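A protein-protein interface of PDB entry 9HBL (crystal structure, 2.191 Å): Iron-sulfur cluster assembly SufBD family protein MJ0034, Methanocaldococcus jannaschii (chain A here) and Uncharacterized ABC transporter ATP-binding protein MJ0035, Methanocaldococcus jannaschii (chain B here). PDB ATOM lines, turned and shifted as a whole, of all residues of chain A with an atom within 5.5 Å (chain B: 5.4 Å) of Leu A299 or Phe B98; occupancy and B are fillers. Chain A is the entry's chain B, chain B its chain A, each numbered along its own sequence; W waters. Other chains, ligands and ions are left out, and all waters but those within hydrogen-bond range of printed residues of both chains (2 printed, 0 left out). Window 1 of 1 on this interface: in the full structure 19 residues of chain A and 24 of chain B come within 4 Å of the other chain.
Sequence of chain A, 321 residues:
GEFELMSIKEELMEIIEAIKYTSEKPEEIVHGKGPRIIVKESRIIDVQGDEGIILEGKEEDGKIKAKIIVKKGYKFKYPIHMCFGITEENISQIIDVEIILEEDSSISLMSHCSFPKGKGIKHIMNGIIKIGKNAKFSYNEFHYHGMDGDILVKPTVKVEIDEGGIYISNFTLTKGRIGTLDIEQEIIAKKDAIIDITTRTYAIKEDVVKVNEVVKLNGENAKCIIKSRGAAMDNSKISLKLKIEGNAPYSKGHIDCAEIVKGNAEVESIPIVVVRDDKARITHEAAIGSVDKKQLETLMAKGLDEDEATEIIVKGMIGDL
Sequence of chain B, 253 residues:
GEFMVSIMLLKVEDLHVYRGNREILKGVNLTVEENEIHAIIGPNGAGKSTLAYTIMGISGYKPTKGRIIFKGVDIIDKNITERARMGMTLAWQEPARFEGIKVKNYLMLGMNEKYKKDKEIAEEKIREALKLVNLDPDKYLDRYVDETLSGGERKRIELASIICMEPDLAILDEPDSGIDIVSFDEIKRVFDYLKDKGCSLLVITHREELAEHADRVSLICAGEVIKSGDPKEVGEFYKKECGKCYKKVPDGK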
ATOM      1  N   LYS A 294     -21.656 -20.452   2.351  1.00  0.00           N
ATOM      2  CA  LYS A 294     -22.691 -20.742   1.370  1.00  0.00           C
ATOM      3  C   LYS A 294     -23.428 -19.469   0.952  1.00  0.00           C
ATOM      4  O   LYS A 294     -23.760 -19.322  -0.217  1.00  0.00           O
ATOM      5  CB  LYS A 294     -23.668 -21.798   1.899  1.00  0.00           C
ATOM      6  CG  LYS A 294     -24.629 -22.314   0.851  1.00  0.00           C
ATOM      7  CD  LYS A 294     -25.431 -23.437   1.423  1.00  0.00           C
ATOM      8  CE  LYS A 294     -26.574 -23.827   0.540  1.00  0.00           C
ATOM      9  NZ  LYS A 294     -27.362 -24.917   1.149  1.00  0.00           N
ATOM     10  N   GLN A 295     -23.670 -18.562   1.882  1.00  0.00           N
ATOM     11  CA  GLN A 295     -24.342 -17.309   1.581  1.00  0.00           C
ATOM     12  C   GLN A 295     -23.482 -16.468   0.640  1.00  0.00           C
ATOM     13  O   GLN A 295     -23.991 -15.886  -0.320  1.00  0.00           O
ATOM     14  CB  GLN A 295     -24.588 -16.516   2.876  1.00  0.00           C
ATOM     15  CG  GLN A 295     -25.851 -16.922   3.578  1.00  0.00           C
ATOM     16  CD  GLN A 295     -25.969 -16.270   4.919  1.00  0.00           C
ATOM     17  OE1 GLN A 295     -25.555 -15.120   5.133  1.00  0.00           O
ATOM     18  NE2 GLN A 295     -26.569 -16.990   5.845  1.00  0.00           N
ATOM     19  N   LEU A 296     -22.173 -16.389   0.943  1.00  0.00           N
ATOM     20  CA  LEU A 296     -21.204 -15.612   0.194  1.00  0.00           C
ATOM     21  C   LEU A 296     -21.112 -16.171  -1.221  1.00  0.00           C
ATOM     22  O   LEU A 296     -21.278 -15.421  -2.180  1.00  0.00           O
ATOM     23  CB  LEU A 296     -19.849 -15.688   0.917  1.00  0.00           C
ATOM     24  CG  LEU A 296     -18.714 -14.941   0.263  1.00  0.00           C
ATOM     25  CD1 LEU A 296     -18.962 -13.449   0.281  1.00  0.00           C
ATOM     26  CD2 LEU A 296     -17.419 -15.263   0.928  1.00  0.00           C
ATOM     27  N   GLU A 297     -20.925 -17.492  -1.350  1.00  0.00           N
ATOM     28  CA  GLU A 297     -20.795 -18.180  -2.625  1.00  0.00           C
ATOM     29  C   GLU A 297     -22.053 -18.160  -3.457  1.00  0.00           C
ATOM     30  O   GLU A 297     -21.961 -18.181  -4.667  1.00  0.00           O
ATOM     31  CB  GLU A 297     -20.287 -19.603  -2.412  1.00  0.00           C
ATOM     32  CG  GLU A 297     -18.900 -19.577  -1.802  1.00  0.00           C
ATOM     33  CD  GLU A 297     -18.149 -20.881  -1.795  1.00  0.00           C
ATOM     34  OE1 GLU A 297     -18.741 -21.920  -1.425  1.00  0.00           O
ATOM     35  OE2 GLU A 297     -16.940 -20.854  -2.119  1.00  0.00           O
ATOM     36  N   THR A 298     -23.222 -18.099  -2.829  1.00  0.00           N
ATOM     37  CA  THR A 298     -24.497 -18.009  -3.537  1.00  0.00           C
ATOM     38  C   THR A 298     -24.587 -16.639  -4.201  1.00  0.00           C
ATOM     39  O   THR A 298     -25.016 -16.561  -5.351  1.00  0.00           O
ATOM     40  CB  THR A 298     -25.691 -18.252  -2.593  1.00  0.00           C
ATOM     41  OG1 THR A 298     -25.628 -19.598  -2.148  1.00  0.00           O
ATOM     42  CG2 THR A 298     -27.040 -18.013  -3.283  1.00  0.00           C
ATOM     43  N   LEU A 299     -24.202 -15.564  -3.482  1.00  0.00           N
ATOM     44  CA  LEU A 299     -24.238 -14.221  -4.061  1.00  0.00           C
ATOM     45  C   LEU A 299     -23.156 -14.041  -5.141  1.00  0.00           C
ATOM     46  O   LEU A 299     -23.417 -13.407  -6.161  1.00  0.00           O
ATOM     47  CB  LEU A 299     -24.153 -13.141  -2.985  1.00  0.00           C
ATOM     48  CG  LEU A 299     -25.314 -13.105  -1.979  1.00  0.00           C
ATOM     49  CD1 LEU A 299     -25.185 -11.920  -1.040  1.00  0.00           C
ATOM     50  CD2 LEU A 299     -26.691 -13.038  -2.671  1.00  0.00           C
ATOM     51  N   MET A 300     -21.975 -14.668  -4.966  1.00  0.00           N
ATOM     52  CA  MET A 300     -20.925 -14.602  -5.972  1.00  0.00           C
ATOM     53  C   MET A 300     -21.317 -15.346  -7.262  1.00  0.00           C
ATOM     54  O   MET A 300     -20.840 -14.995  -8.342  1.00  0.00           O
ATOM     55  CB  MET A 300     -19.607 -15.100  -5.408  1.00  0.00           C
ATOM     56  CG  MET A 300     -19.195 -14.353  -4.156  1.00  0.00           C
ATOM     57  SD  MET A 300     -17.484 -14.640  -3.642  1.00  0.00           S
ATOM     58  CE  MET A 300     -17.492 -16.336  -3.389  1.00  0.00           C
ATOM     59  N   ALA A 301     -22.204 -16.355  -7.168  1.00  0.00           N
ATOM     60  CA  ALA A 301     -22.711 -17.083  -8.341  1.00  0.00           C
ATOM     61  C   ALA A 301     -23.721 -16.227  -9.149  1.00  0.00           C
ATOM     62  O   ALA A 301     -24.055 -16.594 -10.269  1.00  0.00           O
ATOM     63  CB  ALA A 301     -23.332 -18.400  -7.924  1.00  0.00           C
ATOM     64  N   LYS A 302     -24.186 -15.085  -8.579  1.00  0.00           N
ATOM     65  CA  LYS A 302     -25.011 -14.058  -9.209  1.00  0.00           C
ATOM     66  C   LYS A 302     -24.116 -12.978  -9.919  1.00  0.00           C
ATOM     67  O   LYS A 302     -24.649 -11.999 -10.426  1.00  0.00           O
ATOM     68  CB  LYS A 302     -25.878 -13.313  -8.165  1.00  0.00           C
ATOM     69  CG  LYS A 302     -26.605 -14.172  -7.141  1.00  0.00           C
ATOM     70  CD  LYS A 302     -27.755 -14.901  -7.756  1.00  0.00           C
ATOM     71  CE  LYS A 302     -28.358 -15.900  -6.823  1.00  0.00           C
ATOM     72  NZ  LYS A 302     -29.107 -16.930  -7.578  1.00  0.00           N
ATOM     73  N   GLY A 303     -22.790 -13.104  -9.870  1.00  0.00           N
ATOM     74  CA  GLY A 303     -21.888 -12.139 -10.478  1.00  0.00           C
ATOM     75  C   GLY A 303     -21.359 -11.071  -9.545  1.00  0.00           C
ATOM     76  O   GLY A 303     -20.589 -10.220  -9.981  1.00  0.00           O
ATOM     77  N   LEU A 304     -21.762 -11.076  -8.267  1.00  0.00           N
ATOM     78  CA  LEU A 304     -21.253 -10.104  -7.302  1.00  0.00           C
ATOM     79  C   LEU A 304     -19.841 -10.499  -6.857  1.00  0.00           C
ATOM     80  O   LEU A 304     -19.580 -11.692  -6.707  1.00  0.00           O
ATOM     81  CB  LEU A 304     -22.150 -10.066  -6.074  1.00  0.00           C
ATOM     82  CG  LEU A 304     -23.454  -9.292  -6.182  1.00  0.00           C
ATOM     83  CD1 LEU A 304     -24.551 -10.050  -6.950  1.00  0.00           C
ATOM     84  CD2 LEU A 304     -23.948  -8.969  -4.853  1.00  0.00           C
ATOM     85  N   ALA A 309     -20.771  -8.928  -2.246  1.00  0.00           N
ATOM     86  CA  ALA A 309     -21.539  -9.985  -1.603  1.00  0.00           C
ATOM     87  C   ALA A 309     -21.528  -9.849  -0.085  1.00  0.00           C
ATOM     88  O   ALA A 309     -22.576  -9.994   0.542  1.00  0.00           O
ATOM     89  CB  ALA A 309     -21.005 -11.343  -2.014  1.00  0.00           C
ATOM     90  N   ILE A 312     -23.627  -6.866   0.953  1.00  0.00           N
ATOM     91  CA  ILE A 312     -25.044  -7.197   0.864  1.00  0.00           C
ATOM     92  C   ILE A 312     -25.518  -7.951   2.102  1.00  0.00           C
ATOM     93  O   ILE A 312     -26.559  -7.607   2.659  1.00  0.00           O
ATOM     94  CB  ILE A 312     -25.341  -7.948  -0.473  1.00  0.00           C
ATOM     95  CG1 ILE A 312     -25.236  -6.987  -1.668  1.00  0.00           C
ATOM     96  CG2 ILE A 312     -26.713  -8.610  -0.473  1.00  0.00           C
ATOM     97  CD1 ILE A 312     -26.086  -5.647  -1.505  1.00  0.00           C
ATOM     98  N   ILE A 313     -24.739  -8.956   2.536  1.00  0.00           N
ATOM     99  CA  ILE A 313     -25.003  -9.767   3.729  1.00  0.00           C
ATOM    100  C   ILE A 313     -25.027  -8.912   4.986  1.00  0.00           C
ATOM    101  O   ILE A 313     -25.972  -9.004   5.763  1.00  0.00           O
ATOM    102  CB  ILE A 313     -23.994 -10.937   3.836  1.00  0.00           C
ATOM    103  CG1 ILE A 313     -24.294 -11.981   2.753  1.00  0.00           C
ATOM    104  CG2 ILE A 313     -23.989 -11.567   5.240  1.00  0.00           C
ATOM    105  CD1 ILE A 313     -23.147 -12.802   2.413  1.00  0.00           C
ATOM    106  N   ALA B  96     -29.584 -20.957  -0.031  1.00  0.00           N
ATOM    107  CA  ALA B  96     -29.186 -20.290   1.198  1.00  0.00           C
ATOM    108  C   ALA B  96     -30.200 -19.272   1.672  1.00  0.00           C
ATOM    109  O   ALA B  96     -30.767 -18.550   0.860  1.00  0.00           O
ATOM    110  CB  ALA B  96     -27.834 -19.616   1.016  1.00  0.00           C
ATOM    111  N   ARG B  97     -30.449 -19.224   2.979  1.00  0.00           N
ATOM    112  CA  ARG B  97     -31.306 -18.207   3.549  1.00  0.00           C
ATOM    113  C   ARG B  97     -30.407 -17.007   3.871  1.00  0.00           C
ATOM    114  O   ARG B  97     -29.233 -17.178   4.225  1.00  0.00           O
ATOM    115  CB  ARG B  97     -31.987 -18.703   4.835  1.00  0.00           C
ATOM    116  CG  ARG B  97     -32.770 -19.987   4.660  1.00  0.00           C
ATOM    117  CD  ARG B  97     -33.866 -19.869   3.625  1.00  0.00           C
ATOM    118  NE  ARG B  97     -34.558 -21.141   3.464  1.00  0.00           N
ATOM    119  CZ  ARG B  97     -35.789 -21.383   3.894  1.00  0.00           C
ATOM    120  NH1 ARG B  97     -36.496 -20.429   4.478  1.00  0.00           N
ATOM    121  NH2 ARG B  97     -36.329 -22.579   3.731  1.00  0.00           N
ATOM    122  N   PHE B  98     -30.962 -15.793   3.759  1.00  0.00           N
ATOM    123  CA  PHE B  98     -30.240 -14.552   3.985  1.00  0.00           C
ATOM    124  C   PHE B  98     -31.007 -13.680   4.921  1.00  0.00           C
ATOM    125  O   PHE B  98     -32.192 -13.431   4.697  1.00  0.00           O
ATOM    126  CB  PHE B  98     -30.066 -13.780   2.666  1.00  0.00           C
ATOM    127  CG  PHE B  98     -29.164 -14.434   1.645  1.00  0.00           C
ATOM    128  CD1 PHE B  98     -27.807 -14.212   1.659  1.00  0.00           C
ATOM    129  CD2 PHE B  98     -29.684 -15.269   0.674  1.00  0.00           C
ATOM    130  CE1 PHE B  98     -26.985 -14.830   0.736  1.00  0.00           C
ATOM    131  CE2 PHE B  98     -28.857 -15.895  -0.235  1.00  0.00           C
ATOM    132  CZ  PHE B  98     -27.513 -15.672  -0.202  1.00  0.00           C
ATOM    133  N   GLU B  99     -30.326 -13.149   5.939  1.00  0.00           N
ATOM    134  CA  GLU B  99     -30.961 -12.232   6.869  1.00  0.00           C
ATOM    135  C   GLU B  99     -31.136 -10.877   6.179  1.00  0.00           C
ATOM    136  O   GLU B  99     -30.189 -10.368   5.560  1.00  0.00           O
ATOM    137  CB  GLU B  99     -30.088 -12.071   8.133  1.00  0.00           C
ATOM    138  CG  GLU B  99     -30.598 -11.079   9.165  1.00  0.00           C
ATOM    139  CD  GLU B  99     -31.683 -11.609  10.081  1.00  0.00           C
ATOM    140  OE1 GLU B  99     -31.909 -12.840  10.099  1.00  0.00           O
ATOM    141  OE2 GLU B  99     -32.317 -10.786  10.779  1.00  0.00           O
ATOM    142  N   GLY B 100     -32.363 -10.364   6.228  1.00  0.00           N
ATOM    143  CA  GLY B 100     -32.734  -9.037   5.767  1.00  0.00           C
ATOM    144  C   GLY B 100     -32.634  -8.659   4.309  1.00  0.00           C
ATOM    145  O   GLY B 100     -32.598  -7.465   4.008  1.00  0.00           O
ATOM    146  N   ILE B 101     -32.657  -9.629   3.388  1.00  0.00           N
ATOM    147  CA  ILE B 101     -32.642  -9.314   1.958  1.00  0.00           C
ATOM    148  C   ILE B 101     -34.046  -9.569   1.413  1.00  0.00           C
ATOM    149  O   ILE B 101     -34.507 -10.705   1.472  1.00  0.00           O
ATOM    150  CB  ILE B 101     -31.580 -10.145   1.207  1.00  0.00           C
ATOM    151  CG1 ILE B 101     -30.174  -9.863   1.763  1.00  0.00           C
ATOM    152  CG2 ILE B 101     -31.651  -9.888  -0.293  1.00  0.00           C
ATOM    153  CD1 ILE B 101     -29.077 -10.700   1.172  1.00  0.00           C
ATOM    154  N   TYR B 106     -33.400  -9.268  -3.991  1.00  0.00           N
ATOM    155  CA  TYR B 106     -32.682 -10.510  -4.251  1.00  0.00           C
ATOM    156  C   TYR B 106     -32.779 -10.865  -5.742  1.00  0.00           C
ATOM    157  O   TYR B 106     -31.778 -11.277  -6.338  1.00  0.00           O
ATOM    158  CB  TYR B 106     -33.251 -11.656  -3.396  1.00  0.00           C
ATOM    159  CG  TYR B 106     -32.501 -12.955  -3.585  1.00  0.00           C
ATOM    160  CD1 TYR B 106     -31.231 -13.127  -3.052  1.00  0.00           C
ATOM    161  CD2 TYR B 106     -33.048 -14.002  -4.321  1.00  0.00           C
ATOM    162  CE1 TYR B 106     -30.508 -14.292  -3.275  1.00  0.00           C
ATOM    163  CE2 TYR B 106     -32.337 -15.177  -4.540  1.00  0.00           C
ATOM    164  CZ  TYR B 106     -31.066 -15.320  -4.004  1.00  0.00           C
ATOM    165  OH  TYR B 106     -30.334 -16.468  -4.162  1.00  0.00           O
ATOM    166  N   LEU B 109     -30.293  -9.186  -8.179  1.00  0.00           N
ATOM    167  CA  LEU B 109     -28.903  -9.626  -8.157  1.00  0.00           C
ATOM    168  C   LEU B 109     -28.586 -10.563  -9.321  1.00  0.00           C
ATOM    169  O   LEU B 109     -29.168 -11.639  -9.456  1.00  0.00           O
ATOM    170  CB  LEU B 109     -28.561 -10.301  -6.812  1.00  0.00           C
ATOM    171  CG  LEU B 109     -28.908  -9.491  -5.549  1.00  0.00           C
ATOM    172  CD1 LEU B 109     -28.594 -10.263  -4.272  1.00  0.00           C
ATOM    173  CD2 LEU B 109     -28.189  -8.157  -5.545  1.00  0.00           C
ATOM    174  N   TYR B 144     -38.668 -11.323   3.260  1.00  0.00           N
ATOM    175  CA  TYR B 144     -37.227 -11.574   3.299  1.00  0.00           C
ATOM    176  C   TYR B 144     -36.923 -12.987   2.822  1.00  0.00           C
ATOM    177  O   TYR B 144     -37.728 -13.888   3.040  1.00  0.00           O
ATOM    178  CB  TYR B 144     -36.686 -11.346   4.719  1.00  0.00           C
ATOM    179  CG  TYR B 144     -36.790  -9.901   5.137  1.00  0.00           C
ATOM    180  CD1 TYR B 144     -35.969  -8.936   4.575  1.00  0.00           C
ATOM    181  CD2 TYR B 144     -37.766  -9.482   6.027  1.00  0.00           C
ATOM    182  CE1 TYR B 144     -36.070  -7.600   4.932  1.00  0.00           C
ATOM    183  CE2 TYR B 144     -37.877  -8.148   6.397  1.00  0.00           C
ATOM    184  CZ  TYR B 144     -37.033  -7.206   5.837  1.00  0.00           C
ATOM    185  OH  TYR B 144     -37.132  -5.876   6.184  1.00  0.00           O
ATOM    186  N   VAL B 145     -35.768 -13.196   2.181  1.00  0.00           N
ATOM    187  CA  VAL B 145     -35.375 -14.535   1.739  1.00  0.00           C
ATOM    188  C   VAL B 145     -34.642 -15.238   2.883  1.00  0.00           C
ATOM    189  O   VAL B 145     -33.563 -15.780   2.706  1.00  0.00           O
ATOM    190  CB  VAL B 145     -34.586 -14.558   0.403  1.00  0.00           C
ATOM    191  CG1 VAL B 145     -35.511 -14.276  -0.775  1.00  0.00           C
ATOM    192  CG2 VAL B 145     -33.407 -13.589   0.419  1.00  0.00           C
ATOM    193  N   ASP B 146     -35.247 -15.200   4.072  1.00  0.00           N
ATOM    194  CA  ASP B 146     -34.706 -15.732   5.316  1.00  0.00           C
ATOM    195  C   ASP B 146     -35.371 -17.052   5.742  1.00  0.00           C
ATOM    196  O   ASP B 146     -36.131 -17.624   4.961  1.00  0.00           O
ATOM    197  CB  ASP B 146     -34.782 -14.645   6.419  1.00  0.00           C
ATOM    198  CG  ASP B 146     -36.181 -14.166   6.768  1.00  0.00           C
ATOM    199  OD1 ASP B 146     -37.143 -14.615   6.116  1.00  0.00           O
ATOM    200  OD2 ASP B 146     -36.308 -13.320   7.677  1.00  0.00           O
ATOM    201  N   ARG B 154     -38.772 -20.522  -0.800  1.00  0.00           N
ATOM    202  CA  ARG B 154     -37.375 -20.134  -1.033  1.00  0.00           C
ATOM    203  C   ARG B 154     -36.810 -20.751  -2.306  1.00  0.00           C
ATOM    204  O   ARG B 154     -36.095 -20.064  -3.037  1.00  0.00           O
ATOM    205  CB  ARG B 154     -36.492 -20.445   0.182  1.00  0.00           C
ATOM    206  CG  ARG B 154     -35.012 -20.117  -0.012  1.00  0.00           C
ATOM    207  CD  ARG B 154     -34.712 -18.622  -0.049  1.00  0.00           C
ATOM    208  NE  ARG B 154     -33.317 -18.344  -0.416  1.00  0.00           N
ATOM    209  CZ  ARG B 154     -32.870 -18.285  -1.672  1.00  0.00           C
ATOM    210  NH1 ARG B 154     -33.700 -18.490  -2.691  1.00  0.00           N
ATOM    211  NH2 ARG B 154     -31.588 -18.044  -1.916  1.00  0.00           N
HETATM  212  O   HOH W   1     -27.420 -12.806   6.016  1.00  0.00           O
HETATM  213  O   HOH W   2     -27.675 -21.184  -2.159  1.00  0.00           O
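Of the 12 printed residues of chain B, 6 touch a printed residue of chain A.
Hydrophobic or aromatic side chains of chain B within 4 Å of the printed part of chain A: Ala B96, Phe B98, Ile B101, Tyr B106 and Leu B109.
Of the 14 printed residues of chain A, 5 touch a printed residue of chain B.
Hydrophobic or aromatic side chains of chain A within 4 Å of the printed part of chain B: Leu A299 and Ile A312.
Among the printed residues, 10 pairs touch across the chains.
Among the printed residues, no Asp or Glu carboxylate lies within 4 Å of a Lys or Arg side-chain nitrogen of the other chain.
Water W2 bridges OG1 of Thr A298 (2.6 Å) and N of Ala B96 (2.9 Å).
Water W1 lies within hydrogen-bond range of N of Glu B99 (2.9 Å) and OE1 of Gln A295 (3.1 Å).
Of chain B, only Phe B98 (3.6 Å) and Leu B109 (3.7 Å) come within 4 Å of Leu A299.
Phe B98 touches just these residues of chain A: Gln A295, Thr A298 and Leu A299.
Of the printed residues of chain A, Ala B96 touches Thr A298.
Printed residues of chain B within 4 Å of Ile A312: Ile B101.
Printed residues of chain A within 4 Å of Leu B109: Leu A299 and Lys A302.
Of the printed residues of chain A, Tyr B106 touches Thr A298 (3.7 Å) and Lys A302 (3.4 Å).
Asp B146 touches none of the printed residues of chain A.
Glu B99 touches none of the printed residues of chain A.
The nearest residue of chain B that does not touch Leu A299 is Tyr B106 (4.1 Å).
The nearest residue of chain A that does not touch Phe B98 is Ile A313 (4.3 Å).
The nearest printed residue of chain A that does not touch Ile B101 is Leu A299 (4.6 Å).
The guanidinium group of Arg B154 is in hydrogen-bond range of the backbone carbonyl oxygen of Ala B96, 2.9 Å away.
NH1 of Arg B97 sits at hydrogen-bond distance from O of Asp B146.
N of Phe B98 lies within hydrogen-bond range of O of Val B145, 2.8 Å away.
O of Ile B101 is in hydrogen-bond range of N of Val B145.
The guanidinium group (NH2) of Arg B154 sits at hydrogen-bond distance from the side-chain hydroxyl (OH) of Tyr B106.
The backbone carbonyl oxygen (O) of Lys A294 sits at hydrogen-bond distance from the side-chain hydroxyl (OG1) of Thr A298 (2.7 Å).
The backbone carbonyl oxygen (O) of Arg B97 lies within hydrogen-bond range of the side-chain amide nitrogen (NE2) of Gln A295.
Gln A295 touches Phe B98.
Thr A298 touches Ala B96 (OG1 to CB, 3.9 Å).
Phe B98 touches Thr A298 (CZ to CG2, 3.9 Å).
CG2 of Thr A298 touches OH of Tyr B106, at 3.7 Å.
CE1 of Phe B98 touches CG of Leu A299 (3.6 Å).
CD1 of Leu B109 touches CD2 of Leu A299, 3.7 Å away.
Lys A302 touches Tyr B106.
Leu B109 touches Lys A302 (O to CB, 3.9 Å).
Ile A312 touches Ile B101 (CG2 to CD1, 3.6 Å).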
